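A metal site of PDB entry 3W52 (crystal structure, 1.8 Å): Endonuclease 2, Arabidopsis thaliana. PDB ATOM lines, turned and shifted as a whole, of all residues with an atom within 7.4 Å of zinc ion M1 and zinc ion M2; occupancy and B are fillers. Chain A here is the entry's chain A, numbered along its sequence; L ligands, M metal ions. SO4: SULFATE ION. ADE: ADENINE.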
ATOM      1  N   TRP A   1      14.785 -16.845 -10.236  1.00  0.00           N
ATOM      2  CA  TRP A   1      13.485 -16.409  -9.647  1.00  0.00           C
ATOM      3  C   TRP A   1      12.336 -16.932 -10.488  1.00  0.00           C
ATOM      4  O   TRP A   1      12.525 -17.306 -11.647  1.00  0.00           O
ATOM      5  CB  TRP A   1      13.368 -14.845  -9.714  1.00  0.00           C
ATOM      6  CG  TRP A   1      14.524 -14.067  -9.101  1.00  0.00           C
ATOM      7  CD1 TRP A   1      15.616 -13.513  -9.753  1.00  0.00           C
ATOM      8  CD2 TRP A   1      14.646 -13.705  -7.709  1.00  0.00           C
ATOM      9  NE1 TRP A   1      16.395 -12.798  -8.831  1.00  0.00           N
ATOM     10  CE2 TRP A   1      15.829 -12.905  -7.601  1.00  0.00           C
ATOM     11  CE3 TRP A   1      13.894 -13.963  -6.582  1.00  0.00           C
ATOM     12  CZ2 TRP A   1      16.259 -12.385  -6.368  1.00  0.00           C
ATOM     13  CZ3 TRP A   1      14.321 -13.445  -5.329  1.00  0.00           C
ATOM     14  CH2 TRP A   1      15.497 -12.663  -5.245  1.00  0.00           C
ATOM     15  N   GLY A   2      11.160 -16.889  -9.884  1.00  0.00           N
ATOM     16  CA  GLY A   2       9.958 -17.180 -10.640  1.00  0.00           C
ATOM     17  C   GLY A   2       9.506 -15.957 -11.423  1.00  0.00           C
ATOM     18  O   GLY A   2      10.200 -14.934 -11.561  1.00  0.00           O
ATOM     19  N   LYS A   3       8.280 -16.022 -11.935  1.00  0.00           N
ATOM     20  CA  LYS A   3       7.792 -14.922 -12.799  1.00  0.00           C
ATOM     21  C   LYS A   3       7.797 -13.525 -12.194  1.00  0.00           C
ATOM     22  O   LYS A   3       8.212 -12.553 -12.843  1.00  0.00           O
ATOM     23  CB  LYS A   3       6.348 -15.244 -13.258  1.00  0.00           C
ATOM     24  CG  LYS A   3       5.814 -14.295 -14.320  1.00  0.00           C
ATOM     25  CD  LYS A   3       5.737 -15.029 -15.710  1.00  0.00           C
ATOM     26  CE  LYS A   3       5.528 -14.147 -16.982  1.00  0.00           C
ATOM     27  NZ  LYS A   3       6.733 -13.374 -17.415  1.00  0.00           N
ATOM     28  N   GLY A   5       9.559 -12.273  -9.684  1.00  0.00           N
ATOM     29  CA  GLY A   5      10.902 -11.695  -9.475  1.00  0.00           C
ATOM     30  C   GLY A   5      11.487 -11.179 -10.772  1.00  0.00           C
ATOM     31  O   GLY A   5      12.073 -10.075 -10.821  1.00  0.00           O
ATOM     32  N   HIS A   6      11.400 -11.954 -11.851  1.00  0.00           N
ATOM     33  CA  HIS A   6      11.968 -11.461 -13.113  1.00  0.00           C
ATOM     34  C   HIS A   6      11.171 -10.266 -13.638  1.00  0.00           C
ATOM     35  O   HIS A   6      11.733  -9.331 -14.211  1.00  0.00           O
ATOM     36  CB  HIS A   6      11.946 -12.579 -14.184  1.00  0.00           C
ATOM     37  CG  HIS A   6      13.004 -13.604 -13.939  1.00  0.00           C
ATOM     38  ND1 HIS A   6      14.347 -13.328 -14.119  1.00  0.00           N
ATOM     39  CD2 HIS A   6      12.929 -14.827 -13.382  1.00  0.00           C
ATOM     40  CE1 HIS A   6      15.062 -14.353 -13.685  1.00  0.00           C
ATOM     41  NE2 HIS A   6      14.218 -15.277 -13.238  1.00  0.00           N
ATOM     42  N   CYS A  41      10.786 -11.664 -19.796  1.00  0.00           N
ATOM     43  CA  CYS A  41      11.898 -11.963 -18.882  1.00  0.00           C
ATOM     44  C   CYS A  41      11.913 -13.396 -18.330  1.00  0.00           C
ATOM     45  O   CYS A  41      12.877 -13.770 -17.657  1.00  0.00           O
ATOM     46  CB  CYS A  41      11.997 -10.867 -17.788  1.00  0.00           C
ATOM     47  SG  CYS A  41      12.904  -9.461 -18.624  1.00  0.00           S
ATOM     48  N   LEU A  42      10.894 -14.202 -18.652  1.00  0.00           N
ATOM     49  CA  LEU A  42      10.880 -15.628 -18.268  1.00  0.00           C
ATOM     50  C   LEU A  42      11.136 -16.518 -19.497  1.00  0.00           C
ATOM     51  O   LEU A  42      11.202 -17.743 -19.405  1.00  0.00           O
ATOM     52  CB  LEU A  42       9.583 -16.044 -17.602  1.00  0.00           C
ATOM     53  CG  LEU A  42       9.610 -16.981 -16.392  1.00  0.00           C
ATOM     54  CD1 LEU A  42      10.450 -16.462 -15.222  1.00  0.00           C
ATOM     55  CD2 LEU A  42       8.148 -17.098 -15.901  1.00  0.00           C
ATOM     56  N   ALA A  44      13.766 -17.243 -21.034  1.00  0.00           N
ATOM     57  CA  ALA A  44      14.849 -18.220 -20.861  1.00  0.00           C
ATOM     58  C   ALA A  44      14.405 -19.472 -20.134  1.00  0.00           C
ATOM     59  O   ALA A  44      14.882 -20.557 -20.418  1.00  0.00           O
ATOM     60  CB  ALA A  44      16.036 -17.568 -20.101  1.00  0.00           C
ATOM     61  N   ASP A  45      13.504 -19.344 -19.160  1.00  0.00           N
ATOM     62  CA  ASP A  45      13.087 -20.563 -18.465  1.00  0.00           C
ATOM     63  C   ASP A  45      12.289 -21.496 -19.413  1.00  0.00           C
ATOM     64  O   ASP A  45      12.283 -22.712 -19.211  1.00  0.00           O
ATOM     65  CB  ASP A  45      12.208 -20.206 -17.269  1.00  0.00           C
ATOM     66  CG  ASP A  45      13.009 -19.907 -16.017  1.00  0.00           C
ATOM     67  OD1 ASP A  45      14.263 -20.065 -15.982  1.00  0.00           O
ATOM     68  OD2 ASP A  45      12.351 -19.529 -15.011  1.00  0.00           O
ATOM     69  N   LYS A  48      14.618 -24.159 -21.483  1.00  0.00           N
ATOM     70  CA  LYS A  48      15.540 -25.034 -20.737  1.00  0.00           C
ATOM     71  C   LYS A  48      15.594 -26.466 -21.385  1.00  0.00           C
ATOM     72  O   LYS A  48      16.601 -27.146 -21.268  1.00  0.00           O
ATOM     73  CB  LYS A  48      15.025 -25.213 -19.299  1.00  0.00           C
ATOM     74  CG  LYS A  48      15.423 -24.078 -18.378  1.00  0.00           C
ATOM     75  CD  LYS A  48      14.897 -24.296 -16.947  1.00  0.00           C
ATOM     76  CE  LYS A  48      15.422 -23.103 -16.097  1.00  0.00           C
ATOM     77  NZ  LYS A  48      14.746 -23.130 -14.768  1.00  0.00           N
ATOM     78  N   SER A  55      20.310 -25.165 -19.705  1.00  0.00           N
ATOM     79  CA  SER A  55      19.839 -25.366 -18.343  1.00  0.00           C
ATOM     80  C   SER A  55      20.809 -25.012 -17.226  1.00  0.00           C
ATOM     81  O   SER A  55      20.439 -24.317 -16.265  1.00  0.00           O
ATOM     82  CB  SER A  55      19.312 -26.815 -18.154  1.00  0.00           C
ATOM     83  OG  SER A  55      17.959 -26.868 -18.588  1.00  0.00           O
ATOM     84  N   LEU A  57      23.046 -22.862 -17.306  1.00  0.00           N
ATOM     85  CA  LEU A  57      23.401 -21.443 -17.399  1.00  0.00           C
ATOM     86  C   LEU A  57      22.583 -20.601 -16.428  1.00  0.00           C
ATOM     87  O   LEU A  57      22.822 -19.400 -16.361  1.00  0.00           O
ATOM     88  CB  LEU A  57      23.187 -20.907 -18.830  1.00  0.00           C
ATOM     89  CG  LEU A  57      24.026 -21.669 -19.901  1.00  0.00           C
ATOM     90  CD1 LEU A  57      23.792 -20.979 -21.269  1.00  0.00           C
ATOM     91  CD2 LEU A  57      25.520 -21.720 -19.522  1.00  0.00           C
ATOM     92  N   HIS A  58      21.607 -21.187 -15.747  1.00  0.00           N
ATOM     93  CA  HIS A  58      20.785 -20.392 -14.812  1.00  0.00           C
ATOM     94  C   HIS A  58      21.343 -20.289 -13.423  1.00  0.00           C
ATOM     95  O   HIS A  58      20.822 -19.468 -12.621  1.00  0.00           O
ATOM     96  CB  HIS A  58      19.375 -20.995 -14.679  1.00  0.00           C
ATOM     97  CG  HIS A  58      18.594 -20.941 -15.952  1.00  0.00           C
ATOM     98  ND1 HIS A  58      17.448 -20.170 -16.077  1.00  0.00           N
ATOM     99  CD2 HIS A  58      18.821 -21.480 -17.161  1.00  0.00           C
ATOM    100  CE1 HIS A  58      17.005 -20.247 -17.318  1.00  0.00           C
ATOM    101  NE2 HIS A  58      17.820 -21.038 -18.008  1.00  0.00           N
ATOM    102  N   TYR A  59      22.388 -21.061 -13.093  1.00  0.00           N
ATOM    103  CA  TYR A  59      22.841 -20.999 -11.697  1.00  0.00           C
ATOM    104  C   TYR A  59      24.360 -21.321 -11.618  1.00  0.00           C
ATOM    105  O   TYR A  59      24.997 -21.464 -12.655  1.00  0.00           O
ATOM    106  CB  TYR A  59      22.092 -22.013 -10.852  1.00  0.00           C
ATOM    107  CG  TYR A  59      22.160 -23.408 -11.463  1.00  0.00           C
ATOM    108  CD1 TYR A  59      23.264 -24.240 -11.230  1.00  0.00           C
ATOM    109  CD2 TYR A  59      21.134 -23.871 -12.305  1.00  0.00           C
ATOM    110  CE1 TYR A  59      23.368 -25.508 -11.810  1.00  0.00           C
ATOM    111  CE2 TYR A  59      21.240 -25.147 -12.896  1.00  0.00           C
ATOM    112  CZ  TYR A  59      22.360 -25.932 -12.634  1.00  0.00           C
ATOM    113  OH  TYR A  59      22.423 -27.210 -13.214  1.00  0.00           O
ATOM    114  N   HIS A 120      17.225 -12.254 -18.321  1.00  0.00           N
ATOM    115  CA  HIS A 120      16.888 -13.299 -17.347  1.00  0.00           C
ATOM    116  C   HIS A 120      18.099 -13.679 -16.422  1.00  0.00           C
ATOM    117  O   HIS A 120      17.943 -13.803 -15.206  1.00  0.00           O
ATOM    118  CB  HIS A 120      16.431 -14.549 -18.128  1.00  0.00           C
ATOM    119  CG  HIS A 120      15.947 -15.647 -17.239  1.00  0.00           C
ATOM    120  ND1 HIS A 120      14.619 -15.752 -16.864  1.00  0.00           N
ATOM    121  CD2 HIS A 120      16.600 -16.669 -16.642  1.00  0.00           C
ATOM    122  CE1 HIS A 120      14.478 -16.799 -16.057  1.00  0.00           C
ATOM    123  NE2 HIS A 120      15.663 -17.372 -15.904  1.00  0.00           N
ATOM    124  N   PHE A 121      19.270 -13.894 -17.014  1.00  0.00           N
ATOM    125  CA  PHE A 121      20.437 -14.299 -16.233  1.00  0.00           C
ATOM    126  C   PHE A 121      20.926 -13.229 -15.260  1.00  0.00           C
ATOM    127  O   PHE A 121      21.343 -13.558 -14.178  1.00  0.00           O
ATOM    128  CB  PHE A 121      21.581 -14.826 -17.129  1.00  0.00           C
ATOM    129  CG  PHE A 121      21.214 -16.066 -17.901  1.00  0.00           C
ATOM    130  CD1 PHE A 121      20.437 -17.052 -17.334  1.00  0.00           C
ATOM    131  CD2 PHE A 121      21.659 -16.232 -19.213  1.00  0.00           C
ATOM    132  CE1 PHE A 121      20.091 -18.257 -18.058  1.00  0.00           C
ATOM    133  CE2 PHE A 121      21.345 -17.407 -19.938  1.00  0.00           C
ATOM    134  CZ  PHE A 121      20.578 -18.403 -19.370  1.00  0.00           C
ATOM    135  N   GLY A 123      18.974 -11.424 -13.726  1.00  0.00           N
ATOM    136  CA  GLY A 123      18.077 -11.620 -12.632  1.00  0.00           C
ATOM    137  C   GLY A 123      18.489 -12.848 -11.806  1.00  0.00           C
ATOM    138  O   GLY A 123      18.622 -12.769 -10.594  1.00  0.00           O
ATOM    139  N   ASP A 124      18.691 -13.997 -12.458  1.00  0.00           N
ATOM    140  CA  ASP A 124      18.999 -15.216 -11.724  1.00  0.00           C
ATOM    141  C   ASP A 124      20.275 -15.123 -10.891  1.00  0.00           C
ATOM    142  O   ASP A 124      20.344 -15.703  -9.821  1.00  0.00           O
ATOM    143  CB  ASP A 124      19.081 -16.392 -12.709  1.00  0.00           C
ATOM    144  CG  ASP A 124      17.736 -17.046 -12.967  1.00  0.00           C
ATOM    145  OD1 ASP A 124      16.756 -16.576 -12.394  1.00  0.00           O
ATOM    146  OD2 ASP A 124      17.693 -18.036 -13.711  1.00  0.00           O
ATOM    147  N   ILE A 125      21.293 -14.412 -11.408  1.00  0.00           N
ATOM    148  CA  ILE A 125      22.541 -14.352 -10.646  1.00  0.00           C
ATOM    149  C   ILE A 125      22.371 -13.561  -9.338  1.00  0.00           C
ATOM    150  O   ILE A 125      23.257 -13.571  -8.501  1.00  0.00           O
ATOM    151  CB  ILE A 125      23.711 -13.809 -11.488  1.00  0.00           C
ATOM    152  CG1 ILE A 125      25.044 -14.191 -10.826  1.00  0.00           C
ATOM    153  CG2 ILE A 125      23.653 -12.290 -11.600  1.00  0.00           C
ATOM    154  CD1 ILE A 125      26.246 -13.960 -11.858  1.00  0.00           C
ATOM    155  N   GLN A 127      19.569 -14.095  -7.381  1.00  0.00           N
ATOM    156  CA  GLN A 127      18.764 -14.938  -6.447  1.00  0.00           C
ATOM    157  C   GLN A 127      19.839 -15.678  -5.636  1.00  0.00           C
ATOM    158  O   GLN A 127      20.621 -16.450  -6.208  1.00  0.00           O
ATOM    159  CB  GLN A 127      17.877 -15.921  -7.304  1.00  0.00           C
ATOM    160  CG  GLN A 127      16.572 -16.360  -6.601  1.00  0.00           C
ATOM    161  CD  GLN A 127      16.772 -17.405  -5.501  1.00  0.00           C
ATOM    162  OE1 GLN A 127      17.469 -17.175  -4.563  1.00  0.00           O
ATOM    163  NE2 GLN A 127      16.118 -18.561  -5.635  1.00  0.00           N
ATOM    164  N   HIS A 130      20.574 -19.222  -6.337  1.00  0.00           N
ATOM    165  CA  HIS A 130      21.116 -19.610  -7.633  1.00  0.00           C
ATOM    166  C   HIS A 130      22.661 -19.584  -7.614  1.00  0.00           C
ATOM    167  O   HIS A 130      23.285 -19.838  -8.645  1.00  0.00           O
ATOM    168  CB  HIS A 130      20.625 -18.714  -8.763  1.00  0.00           C
ATOM    169  CG  HIS A 130      19.266 -19.124  -9.245  1.00  0.00           C
ATOM    170  ND1 HIS A 130      18.978 -19.384 -10.567  1.00  0.00           N
ATOM    171  CD2 HIS A 130      18.139 -19.381  -8.550  1.00  0.00           C
ATOM    172  CE1 HIS A 130      17.731 -19.801 -10.679  1.00  0.00           C
ATOM    173  NE2 HIS A 130      17.199 -19.806  -9.463  1.00  0.00           N
ATOM    174  N   HIS A 154      14.529 -23.683  -2.189  1.00  0.00           N
ATOM    175  CA  HIS A 154      14.831 -22.973  -3.430  1.00  0.00           C
ATOM    176  C   HIS A 154      13.575 -22.244  -3.938  1.00  0.00           C
ATOM    177  O   HIS A 154      13.640 -21.062  -4.286  1.00  0.00           O
ATOM    178  CB  HIS A 154      15.347 -23.884  -4.528  1.00  0.00           C
ATOM    179  CG  HIS A 154      15.837 -23.136  -5.738  1.00  0.00           C
ATOM    180  ND1 HIS A 154      17.164 -22.777  -5.934  1.00  0.00           N
ATOM    181  CD2 HIS A 154      15.149 -22.592  -6.769  1.00  0.00           C
ATOM    182  CE1 HIS A 154      17.257 -22.062  -7.040  1.00  0.00           C
ATOM    183  NE2 HIS A 154      16.045 -21.925  -7.560  1.00  0.00           N
ATOM    184  N   ASP A 158      12.712 -18.399  -4.922  1.00  0.00           N
ATOM    185  CA  ASP A 158      12.364 -17.970  -6.298  1.00  0.00           C
ATOM    186  C   ASP A 158      10.968 -17.323  -6.300  1.00  0.00           C
ATOM    187  O   ASP A 158      10.728 -16.385  -7.039  1.00  0.00           O
ATOM    188  CB  ASP A 158      12.168 -19.194  -7.219  1.00  0.00           C
ATOM    189  CG  ASP A 158      13.458 -19.660  -7.916  1.00  0.00           C
ATOM    190  OD1 ASP A 158      14.474 -18.953  -7.901  1.00  0.00           O
ATOM    191  OD2 ASP A 158      13.391 -20.788  -8.495  1.00  0.00           O
HETATM  192  S   SO4 L   1      14.623 -20.120 -12.538  1.00  0.00           S
HETATM  193  O1  SO4 L   1      14.756 -18.759 -13.172  1.00  0.00           O
HETATM  194  O2  SO4 L   1      15.752 -20.965 -13.172  1.00  0.00           O
HETATM  195  O3  SO4 L   1      14.659 -20.036 -11.089  1.00  0.00           O
HETATM  196  O4  SO4 L   1      13.247 -20.634 -12.993  1.00  0.00           O
HETATM  197  N9  ADE L   2      17.848 -24.217 -10.043  1.00  0.00           N
HETATM  198  C8  ADE L   2      17.581 -25.383 -10.747  1.00  0.00           C
HETATM  199  N7  ADE L   2      18.489 -26.322 -10.564  1.00  0.00           N
HETATM  200  C5  ADE L   2      19.410 -25.742  -9.700  1.00  0.00           C
HETATM  201  C6  ADE L   2      20.588 -26.225  -9.140  1.00  0.00           C
HETATM  202  N6  ADE L   2      21.043 -27.455  -9.371  1.00  0.00           N
HETATM  203  N1  ADE L   2      21.287 -25.409  -8.326  1.00  0.00           N
HETATM  204  C2  ADE L   2      20.803 -24.148  -8.097  1.00  0.00           C
HETATM  205  N3  ADE L   2      19.701 -23.583  -8.572  1.00  0.00           N
HETATM  206  C4  ADE L   2      19.041 -24.439  -9.382  1.00  0.00           C
HETATM  207 ZN    ZN M   1      14.697 -16.972 -12.263  1.00  0.00          ZN
HETATM  208 ZN    ZN M   2      16.170 -19.068 -14.709  1.00  0.00          ZN
HETATM  209 ZN    ZN M   3      15.358 -20.877  -9.297  1.00  0.00          ZN
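A ring nitrogen (ND1) of His 120 lies within hydrogen-bond range of the backbone carbonyl oxygen (O) of Cys 41.
NZ of Lys 48 lies close to OD1 of Asp 45 (3.3 Å).
The indole nitrogen of Trp 1 is in hydrogen-bond range of the backbone carbonyl oxygen of Gly 123.
The backbone carbonyl oxygen (O) of His 58 lies within hydrogen-bond range of a ring nitrogen (ND1) of His 130.
Within 4 Å of zinc ion M1: Trp 1, His 6, His 120 and Asp 124.
Within 4 Å of zinc ion M2: Asp 45, His 58, His 120 and Asp 124.
Zinc ion M1 is bound by O1 of SO4 L1 (2.0 Å), NE2 of His 6 (2.0 Å), N of Trp 1 (2.0 Å), OD1 of Asp 124 (2.1 Å) and O of Trp 1 (2.3 Å).
Zinc ion M2 is bound by the side-chain carboxylate of Asp 124 (2.1 Å), an oxygen (O1) of SO4 L1 (2.1 Å), a ring nitrogen (NE2) of His 120 (2.1 Å), a ring nitrogen (ND1) of His 58 (2.2 Å), an oxygen (O2) of SO4 L1 (2.5 Å) and the side-chain carboxylate of Asp 45 (2.5 Å).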
